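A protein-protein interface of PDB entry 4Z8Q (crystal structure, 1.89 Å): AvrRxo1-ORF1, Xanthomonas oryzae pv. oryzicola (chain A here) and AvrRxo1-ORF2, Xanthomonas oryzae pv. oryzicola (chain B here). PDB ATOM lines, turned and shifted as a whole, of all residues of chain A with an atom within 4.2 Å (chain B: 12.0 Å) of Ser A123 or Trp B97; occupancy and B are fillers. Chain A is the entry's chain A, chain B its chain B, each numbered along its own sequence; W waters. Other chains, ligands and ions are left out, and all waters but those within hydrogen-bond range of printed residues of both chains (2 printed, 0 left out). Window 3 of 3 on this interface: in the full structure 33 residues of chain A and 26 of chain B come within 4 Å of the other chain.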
ATOM      1  N   PHE A 121     -18.147  12.262  33.043  1.00  0.00           N
ATOM      2  CA  PHE A 121     -18.331  12.866  31.738  1.00  0.00           C
ATOM      3  C   PHE A 121     -17.633  11.997  30.690  1.00  0.00           C
ATOM      4  O   PHE A 121     -16.645  11.336  30.995  1.00  0.00           O
ATOM      5  CB  PHE A 121     -17.755  14.282  31.710  1.00  0.00           C
ATOM      6  CG  PHE A 121     -18.448  15.242  32.633  1.00  0.00           C
ATOM      7  CD1 PHE A 121     -19.805  15.512  32.481  1.00  0.00           C
ATOM      8  CD2 PHE A 121     -17.740  15.901  33.635  1.00  0.00           C
ATOM      9  CE1 PHE A 121     -20.460  16.409  33.336  1.00  0.00           C
ATOM     10  CE2 PHE A 121     -18.385  16.803  34.499  1.00  0.00           C
ATOM     11  CZ  PHE A 121     -19.748  17.059  34.336  1.00  0.00           C
ATOM     12  N   SER A 122     -18.143  11.993  29.464  1.00  0.00           N
ATOM     13  CA  SER A 122     -17.515  11.208  28.401  1.00  0.00           C
ATOM     14  C   SER A 122     -16.337  11.995  27.866  1.00  0.00           C
ATOM     15  O   SER A 122     -16.209  13.190  28.157  1.00  0.00           O
ATOM     16  CB  SER A 122     -18.494  10.985  27.268  1.00  0.00           C
ATOM     17  OG  SER A 122     -18.804  12.220  26.656  1.00  0.00           O
ATOM     18  N   SER A 123     -15.478  11.344  27.085  1.00  0.00           N
ATOM     19  CA  SER A 123     -14.357  12.042  26.474  1.00  0.00           C
ATOM     20  C   SER A 123     -14.853  13.211  25.645  1.00  0.00           C
ATOM     21  O   SER A 123     -14.273  14.294  25.675  1.00  0.00           O
ATOM     22  CB  SER A 123     -13.526  11.091  25.609  1.00  0.00           C
ATOM     23  OG  SER A 123     -12.616  10.385  26.421  1.00  0.00           O
ATOM     24  N   ALA A 124     -15.953  13.003  24.935  1.00  0.00           N
ATOM     25  CA  ALA A 124     -16.505  14.044  24.069  1.00  0.00           C
ATOM     26  C   ALA A 124     -17.066  15.249  24.830  1.00  0.00           C
ATOM     27  O   ALA A 124     -17.051  16.380  24.326  1.00  0.00           O
ATOM     28  CB  ALA A 124     -17.559  13.462  23.155  1.00  0.00           C
ATOM     29  N   GLN A 125     -17.590  15.001  26.025  1.00  0.00           N
ATOM     30  CA  GLN A 125     -18.097  16.073  26.875  1.00  0.00           C
ATOM     31  C   GLN A 125     -16.975  16.974  27.382  1.00  0.00           C
ATOM     32  O   GLN A 125     -17.188  18.182  27.560  1.00  0.00           O
ATOM     33  CB  GLN A 125     -18.855  15.490  28.073  1.00  0.00           C
ATOM     34  CG  GLN A 125     -20.257  14.997  27.751  1.00  0.00           C
ATOM     35  CD  GLN A 125     -20.998  14.510  28.989  1.00  0.00           C
ATOM     36  OE1 GLN A 125     -20.680  13.461  29.537  1.00  0.00           O
ATOM     37  NE2 GLN A 125     -21.977  15.289  29.443  1.00  0.00           N
ATOM     38  N   VAL A 126     -15.801  16.392  27.640  1.00  0.00           N
ATOM     39  CA  VAL A 126     -14.675  17.167  28.180  1.00  0.00           C
ATOM     40  C   VAL A 126     -13.669  17.640  27.131  1.00  0.00           C
ATOM     41  O   VAL A 126     -12.707  18.332  27.474  1.00  0.00           O
ATOM     42  CB  VAL A 126     -13.898  16.418  29.298  1.00  0.00           C
ATOM     43  CG1 VAL A 126     -14.856  15.856  30.333  1.00  0.00           C
ATOM     44  CG2 VAL A 126     -13.044  15.290  28.717  1.00  0.00           C
ATOM     45  N   HIS A 127     -13.881  17.283  25.862  1.00  0.00           N
ATOM     46  CA  HIS A 127     -12.872  17.568  24.828  1.00  0.00           C
ATOM     47  C   HIS A 127     -12.530  19.050  24.643  1.00  0.00           C
ATOM     48  O   HIS A 127     -11.352  19.423  24.634  1.00  0.00           O
ATOM     49  CB  HIS A 127     -13.220  16.960  23.465  1.00  0.00           C
ATOM     50  CG  HIS A 127     -12.191  17.255  22.416  1.00  0.00           C
ATOM     51  ND1 HIS A 127     -10.963  16.627  22.380  1.00  0.00           N
ATOM     52  CD2 HIS A 127     -12.185  18.147  21.394  1.00  0.00           C
ATOM     53  CE1 HIS A 127     -10.254  17.097  21.367  1.00  0.00           C
ATOM     54  NE2 HIS A 127     -10.972  18.027  20.756  1.00  0.00           N
ATOM     55  N   ARG A 207     -10.244   6.599  23.167  1.00  0.00           N
ATOM     56  CA  ARG A 207     -10.865   5.571  22.345  1.00  0.00           C
ATOM     57  C   ARG A 207     -11.772   6.234  21.297  1.00  0.00           C
ATOM     58  O   ARG A 207     -12.990   6.218  21.433  1.00  0.00           O
ATOM     59  CB  ARG A 207     -11.658   4.604  23.242  1.00  0.00           C
ATOM     60  CG  ARG A 207     -10.763   3.678  24.068  1.00  0.00           C
ATOM     61  CD  ARG A 207     -11.466   3.088  25.302  1.00  0.00           C
ATOM     62  NE  ARG A 207     -11.817   4.111  26.293  1.00  0.00           N
ATOM     63  CZ  ARG A 207     -13.059   4.537  26.514  1.00  0.00           C
ATOM     64  NH1 ARG A 207     -14.063   4.023  25.813  1.00  0.00           N
ATOM     65  NH2 ARG A 207     -13.302   5.468  27.435  1.00  0.00           N
ATOM     66  N   PRO A 208     -11.173   6.821  20.243  1.00  0.00           N
ATOM     67  CA  PRO A 208     -11.942   7.532  19.218  1.00  0.00           C
ATOM     68  C   PRO A 208     -12.704   6.569  18.337  1.00  0.00           C
ATOM     69  O   PRO A 208     -12.333   5.390  18.239  1.00  0.00           O
ATOM     70  CB  PRO A 208     -10.859   8.208  18.376  1.00  0.00           C
ATOM     71  CG  PRO A 208      -9.660   7.321  18.539  1.00  0.00           C
ATOM     72  CD  PRO A 208      -9.725   6.913  19.987  1.00  0.00           C
ATOM     73  N   PRO A 209     -13.778   7.053  17.708  1.00  0.00           N
ATOM     74  CA  PRO A 209     -14.523   6.211  16.777  1.00  0.00           C
ATOM     75  C   PRO A 209     -13.826   6.169  15.431  1.00  0.00           C
ATOM     76  O   PRO A 209     -12.852   6.911  15.193  1.00  0.00           O
ATOM     77  CB  PRO A 209     -15.862   6.944  16.651  1.00  0.00           C
ATOM     78  CG  PRO A 209     -15.498   8.384  16.833  1.00  0.00           C
ATOM     79  CD  PRO A 209     -14.412   8.374  17.896  1.00  0.00           C
ATOM     80  N   VAL A 212     -12.482   9.198  13.058  1.00  0.00           N
ATOM     81  CA  VAL A 212     -11.336   9.932  13.588  1.00  0.00           C
ATOM     82  C   VAL A 212     -10.053   9.236  13.131  1.00  0.00           C
ATOM     83  O   VAL A 212      -9.093   9.869  12.671  1.00  0.00           O
ATOM     84  CB  VAL A 212     -11.378   9.971  15.138  1.00  0.00           C
ATOM     85  CG1 VAL A 212     -10.064  10.523  15.723  1.00  0.00           C
ATOM     86  CG2 VAL A 212     -12.564  10.808  15.607  1.00  0.00           C
ATOM     87  N   SER A 330     -15.860   3.077  21.745  1.00  0.00           N
ATOM     88  CA  SER A 330     -15.708   4.484  22.070  1.00  0.00           C
ATOM     89  C   SER A 330     -16.736   4.949  23.105  1.00  0.00           C
ATOM     90  O   SER A 330     -16.462   5.846  23.907  1.00  0.00           O
ATOM     91  CB  SER A 330     -15.888   5.329  20.813  1.00  0.00           C
ATOM     92  OG  SER A 330     -15.430   6.651  21.053  1.00  0.00           O
ATOM     93  N   ASP B  53     -17.837  24.560  12.749  1.00  0.00           N
ATOM     94  CA  ASP B  53     -16.613  25.330  12.687  1.00  0.00           C
ATOM     95  C   ASP B  53     -15.558  24.562  11.881  1.00  0.00           C
ATOM     96  O   ASP B  53     -15.206  23.430  12.223  1.00  0.00           O
ATOM     97  CB  ASP B  53     -16.158  25.597  14.122  1.00  0.00           C
ATOM     98  CG  ASP B  53     -14.735  26.080  14.213  1.00  0.00           C
ATOM     99  OD1 ASP B  53     -14.346  26.984  13.442  1.00  0.00           O
ATOM    100  OD2 ASP B  53     -14.008  25.546  15.078  1.00  0.00           O
ATOM    101  N   THR B  54     -15.078  25.177  10.800  1.00  0.00           N
ATOM    102  CA  THR B  54     -14.078  24.566   9.924  1.00  0.00           C
ATOM    103  C   THR B  54     -12.683  25.083  10.233  1.00  0.00           C
ATOM    104  O   THR B  54     -11.679  24.458   9.882  1.00  0.00           O
ATOM    105  CB  THR B  54     -14.379  24.832   8.450  1.00  0.00           C
ATOM    106  OG1 THR B  54     -14.569  26.237   8.254  1.00  0.00           O
ATOM    107  CG2 THR B  54     -15.632  24.086   8.032  1.00  0.00           C
ATOM    108  N   SER B  55     -12.620  26.245  10.870  1.00  0.00           N
ATOM    109  CA  SER B  55     -11.402  26.618  11.558  1.00  0.00           C
ATOM    110  C   SER B  55     -11.266  25.583  12.669  1.00  0.00           C
ATOM    111  O   SER B  55     -12.260  25.006  13.117  1.00  0.00           O
ATOM    112  CB  SER B  55     -11.504  28.027  12.136  1.00  0.00           C
ATOM    113  OG  SER B  55     -12.447  28.079  13.190  1.00  0.00           O
ATOM    114  N   ASP B  56     -10.041  25.313  13.090  1.00  0.00           N
ATOM    115  CA  ASP B  56      -9.819  24.381  14.187  1.00  0.00           C
ATOM    116  C   ASP B  56      -9.856  25.209  15.472  1.00  0.00           C
ATOM    117  O   ASP B  56      -8.897  25.232  16.240  1.00  0.00           O
ATOM    118  CB  ASP B  56      -8.475  23.667  13.988  1.00  0.00           C
ATOM    119  CG  ASP B  56      -8.172  22.653  15.077  1.00  0.00           C
ATOM    120  OD1 ASP B  56      -9.083  22.324  15.867  1.00  0.00           O
ATOM    121  OD2 ASP B  56      -7.015  22.179  15.138  1.00  0.00           O
ATOM    122  N   ALA B  57     -10.988  25.879  15.691  1.00  0.00           N
ATOM    123  CA  ALA B  57     -11.079  26.980  16.649  1.00  0.00           C
ATOM    124  C   ALA B  57      -9.965  27.997  16.393  1.00  0.00           C
ATOM    125  O   ALA B  57      -9.139  28.269  17.266  1.00  0.00           O
ATOM    126  CB  ALA B  57     -11.046  26.471  18.097  1.00  0.00           C
ATOM    127  N   ARG B  59      -7.335  27.879  14.469  1.00  0.00           N
ATOM    128  CA  ARG B  59      -6.031  27.371  14.044  1.00  0.00           C
ATOM    129  C   ARG B  59      -5.872  27.481  12.538  1.00  0.00           C
ATOM    130  O   ARG B  59      -4.885  28.037  12.037  1.00  0.00           O
ATOM    131  CB  ARG B  59      -5.858  25.908  14.441  1.00  0.00           C
ATOM    132  CG  ARG B  59      -5.038  25.675  15.691  1.00  0.00           C
ATOM    133  CD  ARG B  59      -5.901  25.779  16.923  1.00  0.00           C
ATOM    134  NE  ARG B  59      -5.509  24.798  17.930  1.00  0.00           N
ATOM    135  CZ  ARG B  59      -6.355  24.229  18.782  1.00  0.00           C
ATOM    136  NH1 ARG B  59      -7.646  24.545  18.747  1.00  0.00           N
ATOM    137  NH2 ARG B  59      -5.914  23.344  19.668  1.00  0.00           N
ATOM    138  N   TYR B  70     -11.947  20.162   3.620  1.00  0.00           N
ATOM    139  CA  TYR B  70     -13.299  19.653   3.772  1.00  0.00           C
ATOM    140  C   TYR B  70     -13.977  19.258   2.475  1.00  0.00           C
ATOM    141  O   TYR B  70     -14.741  18.292   2.455  1.00  0.00           O
ATOM    142  CB  TYR B  70     -14.143  20.631   4.577  1.00  0.00           C
ATOM    143  CG  TYR B  70     -13.622  20.695   5.977  1.00  0.00           C
ATOM    144  CD1 TYR B  70     -13.994  19.737   6.913  1.00  0.00           C
ATOM    145  CD2 TYR B  70     -12.700  21.667   6.350  1.00  0.00           C
ATOM    146  CE1 TYR B  70     -13.491  19.767   8.196  1.00  0.00           C
ATOM    147  CE2 TYR B  70     -12.192  21.707   7.631  1.00  0.00           C
ATOM    148  CZ  TYR B  70     -12.594  20.754   8.546  1.00  0.00           C
ATOM    149  OH  TYR B  70     -12.096  20.783   9.818  1.00  0.00           O
ATOM    150  N   MET B  73     -12.290  15.889   1.697  1.00  0.00           N
ATOM    151  CA  MET B  73     -12.762  14.845   2.599  1.00  0.00           C
ATOM    152  C   MET B  73     -14.184  14.421   2.228  1.00  0.00           C
ATOM    153  O   MET B  73     -14.505  13.239   2.179  1.00  0.00           O
ATOM    154  CB  MET B  73     -12.708  15.355   4.035  1.00  0.00           C
ATOM    155  CG  MET B  73     -13.169  14.359   5.053  1.00  0.00           C
ATOM    156  SD  MET B  73     -13.269  15.211   6.833  1.00  0.00           S
ATOM    157  CE  MET B  73     -11.558  16.060   6.711  1.00  0.00           C
ATOM    158  N   TYR B  78     -15.606  10.377   1.897  1.00  0.00           N
ATOM    159  CA  TYR B  78     -16.973   9.964   2.229  1.00  0.00           C
ATOM    160  C   TYR B  78     -17.897   9.976   1.011  1.00  0.00           C
ATOM    161  O   TYR B  78     -18.940  10.656   1.014  1.00  0.00           O
ATOM    162  CB  TYR B  78     -17.546  10.807   3.389  1.00  0.00           C
ATOM    163  CG  TYR B  78     -16.735  10.681   4.673  1.00  0.00           C
ATOM    164  CD1 TYR B  78     -16.950   9.630   5.556  1.00  0.00           C
ATOM    165  CD2 TYR B  78     -15.744  11.600   4.983  1.00  0.00           C
ATOM    166  CE1 TYR B  78     -16.193   9.500   6.731  1.00  0.00           C
ATOM    167  CE2 TYR B  78     -14.990  11.484   6.149  1.00  0.00           C
ATOM    168  CZ  TYR B  78     -15.219  10.432   7.014  1.00  0.00           C
ATOM    169  OH  TYR B  78     -14.464  10.317   8.156  1.00  0.00           O
ATOM    170  N   ALA B  88     -22.075  16.980   8.003  1.00  0.00           N
ATOM    171  CA  ALA B  88     -22.027  17.813   9.191  1.00  0.00           C
ATOM    172  C   ALA B  88     -21.734  16.985  10.409  1.00  0.00           C
ATOM    173  O   ALA B  88     -20.910  17.321  11.182  1.00  0.00           O
ATOM    174  CB  ALA B  88     -23.346  18.498   9.374  1.00  0.00           C
ATOM    175  N   HIS B  89     -22.493  15.929  10.550  1.00  0.00           N
ATOM    176  CA  HIS B  89     -22.381  14.946  11.579  1.00  0.00           C
ATOM    177  C   HIS B  89     -20.939  14.512  11.763  1.00  0.00           C
ATOM    178  O   HIS B  89     -20.454  14.347  12.844  1.00  0.00           O
ATOM    179  CB  HIS B  89     -23.042  13.688  11.057  1.00  0.00           C
ATOM    180  CG  HIS B  89     -24.504  13.553  11.316  1.00  0.00           C
ATOM    181  ND1 HIS B  89     -25.414  13.425  10.293  1.00  0.00           N
ATOM    182  CD2 HIS B  89     -25.202  13.382  12.459  1.00  0.00           C
ATOM    183  CE1 HIS B  89     -26.618  13.258  10.792  1.00  0.00           C
ATOM    184  NE2 HIS B  89     -26.519  13.231  12.105  1.00  0.00           N
ATOM    185  N   ILE B  90     -20.297  14.256  10.642  1.00  0.00           N
ATOM    186  CA  ILE B  90     -18.964  13.693  10.613  1.00  0.00           C
ATOM    187  C   ILE B  90     -17.920  14.653  11.100  1.00  0.00           C
ATOM    188  O   ILE B  90     -17.110  14.319  11.922  1.00  0.00           O
ATOM    189  CB  ILE B  90     -18.638  13.167   9.221  1.00  0.00           C
ATOM    190  CG1 ILE B  90     -19.418  11.903   8.984  1.00  0.00           C
ATOM    191  CG2 ILE B  90     -17.187  12.899   9.085  1.00  0.00           C
ATOM    192  CD1 ILE B  90     -19.348  11.475   7.685  1.00  0.00           C
ATOM    193  N   VAL B  91     -17.955  15.853  10.589  1.00  0.00           N
ATOM    194  CA  VAL B  91     -17.051  16.868  11.013  1.00  0.00           C
ATOM    195  C   VAL B  91     -17.183  17.167  12.485  1.00  0.00           C
ATOM    196  O   VAL B  91     -16.220  17.458  13.119  1.00  0.00           O
ATOM    197  CB  VAL B  91     -17.262  18.127  10.210  1.00  0.00           C
ATOM    198  CG1 VAL B  91     -16.180  19.067  10.459  1.00  0.00           C
ATOM    199  CG2 VAL B  91     -17.334  17.803   8.777  1.00  0.00           C
ATOM    200  N   GLU B  92     -18.404  17.130  12.987  1.00  0.00           N
ATOM    201  CA  GLU B  92     -18.664  17.356  14.409  1.00  0.00           C
ATOM    202  C   GLU B  92     -17.926  16.290  15.213  1.00  0.00           C
ATOM    203  O   GLU B  92     -17.206  16.597  16.171  1.00  0.00           O
ATOM    204  CB  GLU B  92     -20.170  17.296  14.705  1.00  0.00           C
ATOM    205  CG  GLU B  92     -20.909  18.624  14.507  1.00  0.00           C
ATOM    206  CD  GLU B  92     -22.360  18.444  14.069  1.00  0.00           C
ATOM    207  OE1 GLU B  92     -23.041  17.502  14.553  1.00  0.00           O
ATOM    208  OE2 GLU B  92     -22.819  19.251  13.225  1.00  0.00           O
ATOM    209  N   THR B  93     -18.104  15.041  14.795  1.00  0.00           N
ATOM    210  CA  THR B  93     -17.388  13.907  15.374  1.00  0.00           C
ATOM    211  C   THR B  93     -15.881  14.147  15.359  1.00  0.00           C
ATOM    212  O   THR B  93     -15.212  13.964  16.377  1.00  0.00           O
ATOM    213  CB  THR B  93     -17.744  12.614  14.623  1.00  0.00           C
ATOM    214  OG1 THR B  93     -19.162  12.406  14.696  1.00  0.00           O
ATOM    215  CG2 THR B  93     -17.026  11.408  15.218  1.00  0.00           C
ATOM    216  N   LEU B  94     -15.349  14.605  14.227  1.00  0.00           N
ATOM    217  CA  LEU B  94     -13.904  14.744  14.093  1.00  0.00           C
ATOM    218  C   LEU B  94     -13.341  15.760  15.077  1.00  0.00           C
ATOM    219  O   LEU B  94     -12.258  15.565  15.628  1.00  0.00           O
ATOM    220  CB  LEU B  94     -13.503  15.104  12.661  1.00  0.00           C
ATOM    221  CG  LEU B  94     -13.676  14.006  11.609  1.00  0.00           C
ATOM    222  CD1 LEU B  94     -13.086  14.439  10.276  1.00  0.00           C
ATOM    223  CD2 LEU B  94     -13.008  12.744  12.080  1.00  0.00           C
ATOM    224  N   PHE B  95     -14.076  16.841  15.308  1.00  0.00           N
ATOM    225  CA  PHE B  95     -13.596  17.862  16.236  1.00  0.00           C
ATOM    226  C   PHE B  95     -13.929  17.568  17.705  1.00  0.00           C
ATOM    227  O   PHE B  95     -13.465  18.259  18.609  1.00  0.00           O
ATOM    228  CB  PHE B  95     -14.037  19.260  15.782  1.00  0.00           C
ATOM    229  CG  PHE B  95     -13.168  19.830  14.685  1.00  0.00           C
ATOM    230  CD1 PHE B  95     -11.825  19.470  14.601  1.00  0.00           C
ATOM    231  CD2 PHE B  95     -13.686  20.704  13.733  1.00  0.00           C
ATOM    232  CE1 PHE B  95     -11.009  19.982  13.601  1.00  0.00           C
ATOM    233  CE2 PHE B  95     -12.874  21.219  12.728  1.00  0.00           C
ATOM    234  CZ  PHE B  95     -11.532  20.856  12.668  1.00  0.00           C
ATOM    235  N   SER B  96     -14.707  16.518  17.940  1.00  0.00           N
ATOM    236  CA  SER B  96     -14.933  16.029  19.297  1.00  0.00           C
ATOM    237  C   SER B  96     -13.729  15.243  19.795  1.00  0.00           C
ATOM    238  O   SER B  96     -13.639  14.898  20.982  1.00  0.00           O
ATOM    239  CB  SER B  96     -16.163  15.124  19.350  1.00  0.00           C
ATOM    240  OG  SER B  96     -17.349  15.877  19.511  1.00  0.00           O
ATOM    241  N   TRP B  97     -12.821  14.927  18.875  1.00  0.00           N
ATOM    242  CA  TRP B  97     -11.642  14.135  19.196  1.00  0.00           C
ATOM    243  C   TRP B  97     -10.372  14.806  18.699  1.00  0.00           C
ATOM    244  O   TRP B  97     -10.421  15.814  17.997  1.00  0.00           O
ATOM    245  CB  TRP B  97     -11.763  12.725  18.606  1.00  0.00           C
ATOM    246  CG  TRP B  97     -12.944  12.009  19.140  1.00  0.00           C
ATOM    247  CD1 TRP B  97     -14.223  12.092  18.675  1.00  0.00           C
ATOM    248  CD2 TRP B  97     -12.984  11.130  20.276  1.00  0.00           C
ATOM    249  NE1 TRP B  97     -15.054  11.305  19.442  1.00  0.00           N
ATOM    250  CE2 TRP B  97     -14.316  10.710  20.432  1.00  0.00           C
ATOM    251  CE3 TRP B  97     -12.014  10.652  21.168  1.00  0.00           C
ATOM    252  CZ2 TRP B  97     -14.712   9.827  21.443  1.00  0.00           C
ATOM    253  CZ3 TRP B  97     -12.406   9.786  22.170  1.00  0.00           C
ATOM    254  CH2 TRP B  97     -13.743   9.374  22.295  1.00  0.00           C
ATOM    255  N   SER B  98      -9.230  14.255  19.079  1.00  0.00           N
ATOM    256  CA  SER B  98      -7.966  14.754  18.557  1.00  0.00           C
ATOM    257  C   SER B  98      -7.307  13.683  17.701  1.00  0.00           C
ATOM    258  O   SER B  98      -7.974  12.740  17.266  1.00  0.00           O
ATOM    259  CB  SER B  98      -7.040  15.209  19.690  1.00  0.00           C
ATOM    260  OG  SER B  98      -7.271  16.574  20.002  1.00  0.00           O
HETATM  261  O   HOH W   1     -17.293  17.725  21.650  1.00  0.00           O
HETATM  262  O   HOH W   2     -13.057  13.050  23.099  1.00  0.00           O
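A ring nitrogen (NE2) of His A127 lies close to the backbone carbonyl oxygen (O) of Phe B95.
The backbone carbonyl oxygen (O) of Ser B96 lies close to a ring nitrogen (ND1) of His A127 (3.5 Å).
OG of Ser A330 is in hydrogen-bond range of O of Arg A207.
The backbone carbonyl oxygen of His B89 sits at hydrogen-bond distance from the side-chain hydroxyl of Thr B93 (3.0 Å).
O of Glu B92 lies within hydrogen-bond range of OG of Ser B96 (3.4 Å).
Trp B97 touches Ser A123 (CH2 to CB, 3.7 Å).
Trp B97 touches His A127 (C to CE1, 3.5 Å).
His A127 touches Ser B98.
Arg A207 touches Trp B97.
Trp B97 touches Pro A208 (CE3 to CA, 3.7 Å).
CG2 of Thr B93 touches CG of Pro A209 (3.8 Å).
Trp B97 touches Pro A209 (NE1 to CD, 3.4 Å).
Val A212 touches Trp B97 (CG2 to CB, 3.6 Å).
O of Ser B98 touches CG1 of Val A212, at 3.4 Å.
Ser A330 touches Trp B97 (OG to CZ2, 3.3 Å).
Of chain B, only Trp B97 (3.7 Å) comes within 4 Å of Ser A123.
No residue of chain B comes within 4 Å of Ser A122.
No residue of chain B comes within 4 Å of Val A126.
Of chain B, only Phe B95 (3.1 Å), Ser B96 (3.1 Å), Trp B97 (3.5 Å) and Ser B98 (3.3 Å) come within 4 Å of His A127.
Of chain B, only Trp B97 comes within 4 Å of Arg A207.
Pro A208 touches just one residue of chain B: Trp B97 (3.7 Å).
Val A212 touches three residues of chain B.
Of the printed residues of chain B, Ser A330 touches Trp B97.
Of the printed residues of chain A, Phe B95 touches His A127.
Printed residues of chain A within 4 Å of Ser B96: His A127 (3.1 Å).
Of the printed residues of chain A, Leu B94 touches Val A212 (3.6 Å).
Of the printed residues of chain A, Ser B98 touches His A127 (3.3 Å) and Val A212 (3.4 Å).
Printed residues of chain A within 4 Å of Thr B93: Pro A209 (3.8 Å).
Thr B54 touches none of the printed residues of chain A.
The nearest residue of chain B that does not touch Ser A123 is Ser B96 (4.8 Å).
The nearest printed residue of chain A that does not touch Trp B97 is Ala A124 (4.9 Å).
The nearest printed residue of chain A that does not touch Ser B96 is Ala A124 (4.3 Å).
Of the 12 printed residues of chain A, 7 touch a printed residue of chain B.
Hydrophobic or aromatic side chains of chain A that line the printed part of chain B: His A127, Pro A208, Pro A209 and Val A212.
Among the printed residues, no Asp or Glu carboxylate lies within 4 Å of a Lys or Arg side-chain nitrogen of the other chain.
Water W1 lies within hydrogen-bond range of the side-chain hydroxyl (OG) of Ser B96 and the backbone carbonyl oxygen (O) of Ala A124.
Water W2 lies within hydrogen-bond range of O of Ser B96 (2.9 Å), O of Ser A123 (3.1 Å) and N of Ala A124 (3.4 Å).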
